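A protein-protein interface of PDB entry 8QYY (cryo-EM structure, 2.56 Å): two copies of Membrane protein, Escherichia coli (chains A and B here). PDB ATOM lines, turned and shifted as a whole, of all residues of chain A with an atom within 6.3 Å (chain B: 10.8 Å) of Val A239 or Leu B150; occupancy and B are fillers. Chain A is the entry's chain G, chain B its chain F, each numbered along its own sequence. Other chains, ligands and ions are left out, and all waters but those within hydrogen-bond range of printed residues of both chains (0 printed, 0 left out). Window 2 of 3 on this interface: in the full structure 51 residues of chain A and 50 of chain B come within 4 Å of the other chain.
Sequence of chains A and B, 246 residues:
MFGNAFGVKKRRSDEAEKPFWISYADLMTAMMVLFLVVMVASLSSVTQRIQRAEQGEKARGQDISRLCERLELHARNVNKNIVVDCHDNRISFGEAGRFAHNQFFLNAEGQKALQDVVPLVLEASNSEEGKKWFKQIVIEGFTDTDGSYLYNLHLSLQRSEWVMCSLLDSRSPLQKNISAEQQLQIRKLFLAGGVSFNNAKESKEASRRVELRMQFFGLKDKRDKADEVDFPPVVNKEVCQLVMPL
OE1 of Glu A238 sits at hydrogen-bond distance from N of Tyr B149 (2.8 Å).
The side-chain carboxylate of Glu A161 sits close to the backbone NH of His B154 (3.4 Å).
The backbone NH of Leu B150 sits at hydrogen-bond distance from the side-chain carboxylate of Glu A238 (3.0 Å).
The side-chain carboxylate (OE1) of Glu A238 lies close to the side-chain hydroxyl (OG) of Ser B148 (2.3 Å).
The side-chain carboxylate (OE2) of Glu A161 lies close to the backbone carbonyl oxygen (O) of Leu B150 (3.4 Å).
Among the printed residues, merely in contact across the chains: Glu A161 with Leu B153 (3.3 Å), Glu A161 with Leu B157 (3.9 Å), Met A164 with Tyr B149 (3.3 Å), Met A164 with Leu B153 (3.6 Å), Cys A165 with Leu B150 (3.4 Å), Leu A168 with Leu B150 (3.4 Å), Val A239 with Leu B150 (3.8 Å), Gln A241 with Tyr B151 (3.1 Å) and Gln A241 with His B154 (3.2 Å).
No position is printed for both chains.
The backbone carbonyl oxygen of Ser B148 lies within hydrogen-bond range of the side-chain amide nitrogen of Asn B152 (2.7 Å).
A ring nitrogen (NE2) of His B101 sits at hydrogen-bond distance from the side-chain hydroxyl (OH) of Tyr B151 (2.8 Å).
N of Ser A170 sits close to O of Glu A238, 3.3 Å away.
SG of Cys A240 forms a disulfide with SG of Cys A165, 2.0 Å away.
Hydrophobic or aromatic side chains of chain B that line the printed part of chain A: Tyr B149, Leu B150, Tyr B151, Leu B153, His B154 and Leu B157.
Of the 12 printed residues of chain A, 7 touch a printed residue of chain B.
Printed residues of chain A that touch a printed residue of chain B: Glu A161, Met A164, Cys A165, Leu A168, Glu A238, Val A239 and Gln A241.
Hydrophobic or aromatic side chains of chain A that line the printed part of chain B: Met A164 and Leu A168.
Among the printed residues, 14 pairs touch across the chains.
Among the printed residues, no Asp or Glu carboxylate lies within 4 Å of a Lys or Arg side-chain nitrogen of the other chain.
Of the printed residues of chain B, Glu A161 touches Leu B150, Leu B153, His B154 and Leu B157.
Met A164 touches just these residues of chain B: Tyr B149 and Leu B153.
Cys A165 touches just one residue of chain B: Leu B150.
Leu A168 touches one residue of chain B.
Lys A237 touches none of the printed residues of chain B.
Glu A238 touches just these residues of chain B: Ser B148 (2.3 Å), Tyr B149 (2.8 Å) and Leu B150 (3.0 Å).
Val A239 touches one residue of chain B.
No residue of chain B comes within 4 Å of Cys A240.
Of the printed residues of chain A, Tyr B149 touches Met A164 and Glu A238.
Leu B150 touches just these residues of chain A: Glu A161, Cys A165, Leu A168, Glu A238 and Val A239.
Of the printed residues of chain A, Leu B153 touches Glu A161 and Met A164.
Of the printed residues of chain A, Leu B157 touches Glu A161.
The nearest residue of chain A that does not touch Leu B150 is Met A164 (4.1 Å).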
ATOM      1  N   GLU A 161      14.181  -5.006  10.884  1.00  0.00           N
ATOM      2  CA  GLU A 161      14.561  -5.435   9.544  1.00  0.00           C
ATOM      3  C   GLU A 161      16.000  -5.934   9.515  1.00  0.00           C
ATOM      4  O   GLU A 161      16.314  -6.892   8.805  1.00  0.00           O
ATOM      5  CB  GLU A 161      14.360  -4.291   8.550  1.00  0.00           C
ATOM      6  CG  GLU A 161      14.765  -4.630   7.127  1.00  0.00           C
ATOM      7  CD  GLU A 161      13.650  -5.302   6.355  1.00  0.00           C
ATOM      8  OE1 GLU A 161      12.472  -5.068   6.690  1.00  0.00           O
ATOM      9  OE2 GLU A 161      13.955  -6.063   5.413  1.00  0.00           O
ATOM     10  N   MET A 164      15.985  -9.435  11.016  1.00  0.00           N
ATOM     11  CA  MET A 164      15.500 -10.406  10.040  1.00  0.00           C
ATOM     12  C   MET A 164      16.511 -10.638   8.922  1.00  0.00           C
ATOM     13  O   MET A 164      16.691 -11.779   8.477  1.00  0.00           O
ATOM     14  CB  MET A 164      14.161  -9.958   9.461  1.00  0.00           C
ATOM     15  CG  MET A 164      13.286 -11.113   9.005  1.00  0.00           C
ATOM     16  SD  MET A 164      12.859 -12.218  10.364  1.00  0.00           S
ATOM     17  CE  MET A 164      12.644 -13.764   9.488  1.00  0.00           C
ATOM     18  N   CYS A 165      17.173  -9.578   8.454  1.00  0.00           N
ATOM     19  CA  CYS A 165      18.261  -9.730   7.494  1.00  0.00           C
ATOM     20  C   CYS A 165      19.325 -10.669   8.039  1.00  0.00           C
ATOM     21  O   CYS A 165      19.660 -11.684   7.420  1.00  0.00           O
ATOM     22  CB  CYS A 165      18.883  -8.363   7.189  1.00  0.00           C
ATOM     23  SG  CYS A 165      18.042  -7.333   5.975  1.00  0.00           S
ATOM     24  N   SER A 166      19.824 -10.365   9.237  1.00  0.00           N
ATOM     25  CA  SER A 166      20.874 -11.163   9.853  1.00  0.00           C
ATOM     26  C   SER A 166      20.453 -12.616  10.010  1.00  0.00           C
ATOM     27  O   SER A 166      21.289 -13.521   9.918  1.00  0.00           O
ATOM     28  CB  SER A 166      21.229 -10.562  11.209  1.00  0.00           C
ATOM     29  OG  SER A 166      20.349 -11.023  12.220  1.00  0.00           O
ATOM     30  N   LEU A 168      18.368 -14.069   7.854  1.00  0.00           N
ATOM     31  CA  LEU A 168      18.192 -14.631   6.519  1.00  0.00           C
ATOM     32  C   LEU A 168      18.859 -13.785   5.434  1.00  0.00           C
ATOM     33  O   LEU A 168      18.217 -13.442   4.434  1.00  0.00           O
ATOM     34  CB  LEU A 168      16.705 -14.811   6.199  1.00  0.00           C
ATOM     35  CG  LEU A 168      16.351 -15.967   5.261  1.00  0.00           C
ATOM     36  CD1 LEU A 168      17.141 -17.207   5.638  1.00  0.00           C
ATOM     37  CD2 LEU A 168      14.857 -16.247   5.300  1.00  0.00           C
ATOM     38  N   ASP A 169      20.129 -13.433   5.606  1.00  0.00           N
ATOM     39  CA  ASP A 169      20.891 -12.745   4.572  1.00  0.00           C
ATOM     40  C   ASP A 169      21.982 -13.659   4.030  1.00  0.00           C
ATOM     41  O   ASP A 169      22.521 -14.505   4.747  1.00  0.00           O
ATOM     42  CB  ASP A 169      21.518 -11.453   5.105  1.00  0.00           C
ATOM     43  CG  ASP A 169      22.291 -10.694   4.043  1.00  0.00           C
ATOM     44  OD1 ASP A 169      21.907 -10.768   2.858  1.00  0.00           O
ATOM     45  OD2 ASP A 169      23.281 -10.020   4.398  1.00  0.00           O
ATOM     46  N   SER A 170      22.303 -13.479   2.750  1.00  0.00           N
ATOM     47  CA  SER A 170      23.340 -14.283   2.120  1.00  0.00           C
ATOM     48  C   SER A 170      24.697 -13.997   2.751  1.00  0.00           C
ATOM     49  O   SER A 170      24.937 -12.919   3.303  1.00  0.00           O
ATOM     50  CB  SER A 170      23.390 -14.005   0.617  1.00  0.00           C
ATOM     51  OG  SER A 170      24.515 -14.625   0.020  1.00  0.00           O
ATOM     52  N   LYS A 237      19.469 -16.635  -3.552  1.00  0.00           N
ATOM     53  CA  LYS A 237      19.808 -16.225  -2.197  1.00  0.00           C
ATOM     54  C   LYS A 237      19.218 -14.857  -1.872  1.00  0.00           C
ATOM     55  O   LYS A 237      19.103 -13.979  -2.733  1.00  0.00           O
ATOM     56  CB  LYS A 237      21.325 -16.197  -2.012  1.00  0.00           C
ATOM     57  CG  LYS A 237      21.992 -17.551  -2.180  1.00  0.00           C
ATOM     58  CD  LYS A 237      21.534 -18.528  -1.111  1.00  0.00           C
ATOM     59  CE  LYS A 237      22.094 -18.159   0.253  1.00  0.00           C
ATOM     60  NZ  LYS A 237      21.713 -19.154   1.294  1.00  0.00           N
ATOM     61  N   GLU A 238      18.840 -14.684  -0.609  1.00  0.00           N
ATOM     62  CA  GLU A 238      18.267 -13.431  -0.144  1.00  0.00           C
ATOM     63  C   GLU A 238      19.333 -12.345  -0.065  1.00  0.00           C
ATOM     64  O   GLU A 238      20.512 -12.614   0.173  1.00  0.00           O
ATOM     65  CB  GLU A 238      17.618 -13.616   1.230  1.00  0.00           C
ATOM     66  CG  GLU A 238      16.406 -14.533   1.236  1.00  0.00           C
ATOM     67  CD  GLU A 238      15.231 -13.956   0.472  1.00  0.00           C
ATOM     68  OE1 GLU A 238      15.081 -12.717   0.454  1.00  0.00           O
ATOM     69  OE2 GLU A 238      14.455 -14.744  -0.110  1.00  0.00           O
ATOM     70  N   VAL A 239      18.903 -11.103  -0.273  1.00  0.00           N
ATOM     71  CA  VAL A 239      19.773  -9.937  -0.192  1.00  0.00           C
ATOM     72  C   VAL A 239      19.123  -8.916   0.731  1.00  0.00           C
ATOM     73  O   VAL A 239      17.958  -8.551   0.535  1.00  0.00           O
ATOM     74  CB  VAL A 239      20.035  -9.319  -1.580  1.00  0.00           C
ATOM     75  CG1 VAL A 239      20.862  -8.049  -1.451  1.00  0.00           C
ATOM     76  CG2 VAL A 239      20.725 -10.323  -2.492  1.00  0.00           C
ATOM     77  N   CYS A 240      19.868  -8.462   1.735  1.00  0.00           N
ATOM     78  CA  CYS A 240      19.357  -7.442   2.640  1.00  0.00           C
ATOM     79  C   CYS A 240      19.305  -6.093   1.935  1.00  0.00           C
ATOM     80  O   CYS A 240      20.214  -5.742   1.177  1.00  0.00           O
ATOM     81  CB  CYS A 240      20.226  -7.349   3.891  1.00  0.00           C
ATOM     82  SG  CYS A 240      19.552  -6.251   5.155  1.00  0.00           S
ATOM     83  N   GLN A 241      18.239  -5.335   2.186  1.00  0.00           N
ATOM     84  CA  GLN A 241      18.050  -4.049   1.529  1.00  0.00           C
ATOM     85  C   GLN A 241      18.333  -2.856   2.434  1.00  0.00           C
ATOM     86  O   GLN A 241      18.209  -1.715   1.978  1.00  0.00           O
ATOM     87  CB  GLN A 241      16.630  -3.951   0.970  1.00  0.00           C
ATOM     88  CG  GLN A 241      16.380  -4.917  -0.172  1.00  0.00           C
ATOM     89  CD  GLN A 241      14.975  -4.833  -0.720  1.00  0.00           C
ATOM     90  OE1 GLN A 241      14.135  -4.097  -0.203  1.00  0.00           O
ATOM     91  NE2 GLN A 241      14.715  -5.580  -1.784  1.00  0.00           N
ATOM     92  N   HIS B 101       3.790  -3.854  -7.122  1.00  0.00           N
ATOM     93  CA  HIS B 101       5.192  -4.149  -6.859  1.00  0.00           C
ATOM     94  C   HIS B 101       5.988  -2.860  -6.695  1.00  0.00           C
ATOM     95  O   HIS B 101       5.784  -1.887  -7.427  1.00  0.00           O
ATOM     96  CB  HIS B 101       5.777  -4.994  -7.990  1.00  0.00           C
ATOM     97  CG  HIS B 101       7.267  -5.130  -7.932  1.00  0.00           C
ATOM     98  ND1 HIS B 101       8.117  -4.316  -8.651  1.00  0.00           N
ATOM     99  CD2 HIS B 101       8.058  -5.983  -7.240  1.00  0.00           C
ATOM    100  CE1 HIS B 101       9.368  -4.663  -8.404  1.00  0.00           C
ATOM    101  NE2 HIS B 101       9.360  -5.672  -7.552  1.00  0.00           N
ATOM    102  N   THR B 143       1.877  -9.819   2.325  1.00  0.00           N
ATOM    103  CA  THR B 143       2.567  -9.836   1.045  1.00  0.00           C
ATOM    104  C   THR B 143       2.638 -11.278   0.556  1.00  0.00           C
ATOM    105  O   THR B 143       2.600 -12.223   1.348  1.00  0.00           O
ATOM    106  CB  THR B 143       3.973  -9.216   1.167  1.00  0.00           C
ATOM    107  OG1 THR B 143       3.857  -7.869   1.643  1.00  0.00           O
ATOM    108  CG2 THR B 143       4.684  -9.178  -0.178  1.00  0.00           C
ATOM    109  N   ASP B 144       2.728 -11.437  -0.765  1.00  0.00           N
ATOM    110  CA  ASP B 144       2.807 -12.750  -1.384  1.00  0.00           C
ATOM    111  C   ASP B 144       4.018 -13.527  -0.869  1.00  0.00           C
ATOM    112  O   ASP B 144       4.965 -12.968  -0.305  1.00  0.00           O
ATOM    113  CB  ASP B 144       2.887 -12.618  -2.903  1.00  0.00           C
ATOM    114  CG  ASP B 144       1.666 -11.949  -3.497  1.00  0.00           C
ATOM    115  OD1 ASP B 144       0.594 -12.587  -3.529  1.00  0.00           O
ATOM    116  OD2 ASP B 144       1.780 -10.784  -3.931  1.00  0.00           O
ATOM    117  N   THR B 145       3.983 -14.840  -1.076  1.00  0.00           N
ATOM    118  CA  THR B 145       5.075 -15.721  -0.688  1.00  0.00           C
ATOM    119  C   THR B 145       6.187 -15.776  -1.729  1.00  0.00           C
ATOM    120  O   THR B 145       7.242 -16.358  -1.458  1.00  0.00           O
ATOM    121  CB  THR B 145       4.550 -17.136  -0.426  1.00  0.00           C
ATOM    122  OG1 THR B 145       3.727 -17.554  -1.521  1.00  0.00           O
ATOM    123  CG2 THR B 145       3.733 -17.170   0.856  1.00  0.00           C
ATOM    124  N   ASP B 146       5.979 -15.187  -2.900  1.00  0.00           N
ATOM    125  CA  ASP B 146       6.966 -15.179  -3.968  1.00  0.00           C
ATOM    126  C   ASP B 146       7.947 -14.026  -3.783  1.00  0.00           C
ATOM    127  O   ASP B 146       7.770 -13.152  -2.930  1.00  0.00           O
ATOM    128  CB  ASP B 146       6.280 -15.082  -5.336  1.00  0.00           C
ATOM    129  CG  ASP B 146       5.903 -16.438  -5.895  1.00  0.00           C
ATOM    130  OD1 ASP B 146       6.790 -17.311  -5.986  1.00  0.00           O
ATOM    131  OD2 ASP B 146       4.718 -16.629  -6.244  1.00  0.00           O
ATOM    132  N   GLY B 147       8.994 -14.036  -4.601  1.00  0.00           N
ATOM    133  CA  GLY B 147      10.009 -13.006  -4.542  1.00  0.00           C
ATOM    134  C   GLY B 147      10.944 -13.189  -3.364  1.00  0.00           C
ATOM    135  O   GLY B 147      10.880 -14.162  -2.611  1.00  0.00           O
ATOM    136  N   SER B 148      11.837 -12.217  -3.206  1.00  0.00           N
ATOM    137  CA  SER B 148      12.766 -12.235  -2.086  1.00  0.00           C
ATOM    138  C   SER B 148      12.014 -11.990  -0.784  1.00  0.00           C
ATOM    139  O   SER B 148      11.207 -11.061  -0.686  1.00  0.00           O
ATOM    140  CB  SER B 148      13.855 -11.181  -2.281  1.00  0.00           C
ATOM    141  OG  SER B 148      14.750 -11.160  -1.182  1.00  0.00           O
ATOM    142  N   TYR B 149      12.274 -12.836   0.216  1.00  0.00           N
ATOM    143  CA  TYR B 149      11.598 -12.691   1.501  1.00  0.00           C
ATOM    144  C   TYR B 149      11.943 -11.363   2.160  1.00  0.00           C
ATOM    145  O   TYR B 149      11.063 -10.679   2.697  1.00  0.00           O
ATOM    146  CB  TYR B 149      11.963 -13.859   2.420  1.00  0.00           C
ATOM    147  CG  TYR B 149      11.416 -13.734   3.824  1.00  0.00           C
ATOM    148  CD1 TYR B 149      10.131 -14.159   4.130  1.00  0.00           C
ATOM    149  CD2 TYR B 149      12.192 -13.206   4.850  1.00  0.00           C
ATOM    150  CE1 TYR B 149       9.628 -14.050   5.414  1.00  0.00           C
ATOM    151  CE2 TYR B 149      11.699 -13.092   6.134  1.00  0.00           C
ATOM    152  CZ  TYR B 149      10.417 -13.517   6.411  1.00  0.00           C
ATOM    153  OH  TYR B 149       9.923 -13.407   7.691  1.00  0.00           O
ATOM    154  N   LEU B 150      13.219 -10.976   2.123  1.00  0.00           N
ATOM    155  CA  LEU B 150      13.615  -9.718   2.745  1.00  0.00           C
ATOM    156  C   LEU B 150      13.054  -8.528   1.978  1.00  0.00           C
ATOM    157  O   LEU B 150      12.689  -7.512   2.581  1.00  0.00           O
ATOM    158  CB  LEU B 150      15.136  -9.630   2.851  1.00  0.00           C
ATOM    159  CG  LEU B 150      15.709 -10.108   4.188  1.00  0.00           C
ATOM    160  CD1 LEU B 150      15.227  -9.205   5.312  1.00  0.00           C
ATOM    161  CD2 LEU B 150      15.366 -11.563   4.471  1.00  0.00           C
ATOM    162  N   TYR B 151      12.973  -8.635   0.649  1.00  0.00           N
ATOM    163  CA  TYR B 151      12.331  -7.591  -0.146  1.00  0.00           C
ATOM    164  C   TYR B 151      10.878  -7.406   0.273  1.00  0.00           C
ATOM    165  O   TYR B 151      10.424  -6.279   0.502  1.00  0.00           O
ATOM    166  CB  TYR B 151      12.426  -7.940  -1.633  1.00  0.00           C
ATOM    167  CG  TYR B 151      11.744  -6.960  -2.570  1.00  0.00           C
ATOM    168  CD1 TYR B 151      11.664  -5.605  -2.268  1.00  0.00           C
ATOM    169  CD2 TYR B 151      11.176  -7.397  -3.760  1.00  0.00           C
ATOM    170  CE1 TYR B 151      11.042  -4.717  -3.124  1.00  0.00           C
ATOM    171  CE2 TYR B 151      10.553  -6.515  -4.621  1.00  0.00           C
ATOM    172  CZ  TYR B 151      10.489  -5.177  -4.299  1.00  0.00           C
ATOM    173  OH  TYR B 151       9.869  -4.298  -5.155  1.00  0.00           O
ATOM    174  N   ASN B 152      10.135  -8.510   0.382  1.00  0.00           N
ATOM    175  CA  ASN B 152       8.732  -8.423   0.773  1.00  0.00           C
ATOM    176  C   ASN B 152       8.586  -7.848   2.174  1.00  0.00           C
ATOM    177  O   ASN B 152       7.722  -6.995   2.418  1.00  0.00           O
ATOM    178  CB  ASN B 152       8.085  -9.806   0.691  1.00  0.00           C
ATOM    179  CG  ASN B 152       8.165 -10.403  -0.699  1.00  0.00           C
ATOM    180  OD1 ASN B 152       7.847  -9.746  -1.689  1.00  0.00           O
ATOM    181  ND2 ASN B 152       8.597 -11.656  -0.780  1.00  0.00           N
ATOM    182  N   LEU B 153       9.426  -8.298   3.109  1.00  0.00           N
ATOM    183  CA  LEU B 153       9.346  -7.798   4.477  1.00  0.00           C
ATOM    184  C   LEU B 153       9.643  -6.306   4.538  1.00  0.00           C
ATOM    185  O   LEU B 153       8.912  -5.549   5.188  1.00  0.00           O
ATOM    186  CB  LEU B 153      10.309  -8.565   5.378  1.00  0.00           C
ATOM    187  CG  LEU B 153      10.401  -7.992   6.791  1.00  0.00           C
ATOM    188  CD1 LEU B 153       9.292  -8.555   7.664  1.00  0.00           C
ATOM    189  CD2 LEU B 153      11.766  -8.257   7.397  1.00  0.00           C
ATOM    190  N   HIS B 154      10.711  -5.865   3.868  1.00  0.00           N
ATOM    191  CA  HIS B 154      11.057  -4.449   3.878  1.00  0.00           C
ATOM    192  C   HIS B 154       9.964  -3.613   3.230  1.00  0.00           C
ATOM    193  O   HIS B 154       9.618  -2.538   3.730  1.00  0.00           O
ATOM    194  CB  HIS B 154      12.394  -4.226   3.172  1.00  0.00           C
ATOM    195  CG  HIS B 154      12.773  -2.784   3.037  1.00  0.00           C
ATOM    196  ND1 HIS B 154      13.025  -1.975   4.123  1.00  0.00           N
ATOM    197  CD2 HIS B 154      12.938  -2.006   1.941  1.00  0.00           C
ATOM    198  CE1 HIS B 154      13.331  -0.760   3.704  1.00  0.00           C
ATOM    199  NE2 HIS B 154      13.284  -0.752   2.384  1.00  0.00           N
ATOM    200  N   LEU B 155       9.396  -4.097   2.123  1.00  0.00           N
ATOM    201  CA  LEU B 155       8.344  -3.348   1.445  1.00  0.00           C
ATOM    202  C   LEU B 155       7.116  -3.207   2.340  1.00  0.00           C
ATOM    203  O   LEU B 155       6.582  -2.105   2.504  1.00  0.00           O
ATOM    204  CB  LEU B 155       7.994  -4.032   0.121  1.00  0.00           C
ATOM    205  CG  LEU B 155       7.049  -3.339  -0.869  1.00  0.00           C
ATOM    206  CD1 LEU B 155       7.368  -3.800  -2.281  1.00  0.00           C
ATOM    207  CD2 LEU B 155       5.587  -3.613  -0.554  1.00  0.00           C
ATOM    208  N   SER B 156       6.665  -4.311   2.943  1.00  0.00           N
ATOM    209  CA  SER B 156       5.488  -4.253   3.806  1.00  0.00           C
ATOM    210  C   SER B 156       5.739  -3.388   5.035  1.00  0.00           C
ATOM    211  O   SER B 156       4.853  -2.641   5.472  1.00  0.00           O
ATOM    212  CB  SER B 156       5.070  -5.663   4.222  1.00  0.00           C
ATOM    213  OG  SER B 156       4.604  -6.405   3.109  1.00  0.00           O
ATOM    214  N   LEU B 157       6.939  -3.475   5.611  1.00  0.00           N
ATOM    215  CA  LEU B 157       7.252  -2.665   6.780  1.00  0.00           C
ATOM    216  C   LEU B 157       7.298  -1.187   6.410  1.00  0.00           C
ATOM    217  O   LEU B 157       6.894  -0.324   7.200  1.00  0.00           O
ATOM    218  CB  LEU B 157       8.580  -3.123   7.380  1.00  0.00           C
ATOM    219  CG  LEU B 157       8.985  -2.469   8.694  1.00  0.00           C
ATOM    220  CD1 LEU B 157       7.954  -2.847   9.741  1.00  0.00           C
ATOM    221  CD2 LEU B 157      10.378  -2.906   9.115  1.00  0.00           C
ATOM    222  N   GLN B 158       7.780  -0.878   5.203  1.00  0.00           N
ATOM    223  CA  GLN B 158       7.740   0.490   4.704  1.00  0.00           C
ATOM    224  C   GLN B 158       6.306   0.966   4.522  1.00  0.00           C
ATOM    225  O   GLN B 158       5.989   2.126   4.803  1.00  0.00           O
ATOM    226  CB  GLN B 158       8.512   0.579   3.388  1.00  0.00           C
ATOM    227  CG  GLN B 158       8.622   1.976   2.817  1.00  0.00           C
ATOM    228  CD  GLN B 158       9.442   2.025   1.544  1.00  0.00           C
ATOM    229  OE1 GLN B 158       9.660   3.095   0.974  1.00  0.00           O
ATOM    230  NE2 GLN B 158       9.901   0.866   1.090  1.00  0.00           N
ATOM    231  N   ARG B 159       5.426   0.085   4.038  1.00  0.00           N
ATOM    232  CA  ARG B 159       4.008   0.427   3.943  1.00  0.00           C
ATOM    233  C   ARG B 159       3.443   0.772   5.313  1.00  0.00           C
ATOM    234  O   ARG B 159       2.710   1.756   5.470  1.00  0.00           O
ATOM    235  CB  ARG B 159       3.221  -0.734   3.333  1.00  0.00           C
ATOM    236  CG  ARG B 159       3.778  -1.287   2.043  1.00  0.00           C
ATOM    237  CD  ARG B 159       2.675  -1.624   1.068  1.00  0.00           C
ATOM    238  NE  ARG B 159       1.707  -2.543   1.653  1.00  0.00           N
ATOM    239  CZ  ARG B 159       1.794  -3.864   1.592  1.00  0.00           C
ATOM    240  NH1 ARG B 159       2.800  -4.465   0.979  1.00  0.00           N
ATOM    241  NH2 ARG B 159       0.846  -4.604   2.163  1.00  0.00           N
ATOM    242  N   VAL B 195       4.556  -8.624  10.169  1.00  0.00           N
ATOM    243  CA  VAL B 195       4.282  -8.850   8.756  1.00  0.00           C
ATOM    244  C   VAL B 195       3.855 -10.300   8.575  1.00  0.00           C
ATOM    245  O   VAL B 195       4.550 -11.219   9.026  1.00  0.00           O
ATOM    246  CB  VAL B 195       5.507  -8.522   7.885  1.00  0.00           C
ATOM    247  CG1 VAL B 195       5.355  -9.130   6.500  1.00  0.00           C
ATOM    248  CG2 VAL B 195       5.702  -7.017   7.790  1.00  0.00           C
ATOM    249  N   PHE B 197       2.256 -13.461   5.896  1.00  0.00           N
ATOM    250  CA  PHE B 197       2.389 -13.968   4.533  1.00  0.00           C
ATOM    251  C   PHE B 197       1.264 -14.943   4.213  1.00  0.00           C
ATOM    252  O   PHE B 197       1.483 -16.044   3.705  1.00  0.00           O
ATOM    253  CB  PHE B 197       3.749 -14.627   4.322  1.00  0.00           C
ATOM    254  CG  PHE B 197       4.909 -13.675   4.405  1.00  0.00           C
ATOM    255  CD1 PHE B 197       5.413 -13.276   5.632  1.00  0.00           C
ATOM    256  CD2 PHE B 197       5.497 -13.178   3.251  1.00  0.00           C
ATOM    257  CE1 PHE B 197       6.480 -12.401   5.707  1.00  0.00           C
ATOM    258  CE2 PHE B 197       6.563 -12.302   3.321  1.00  0.00           C
ATOM    259  CZ  PHE B 197       7.056 -11.913   4.550  1.00  0.00           C
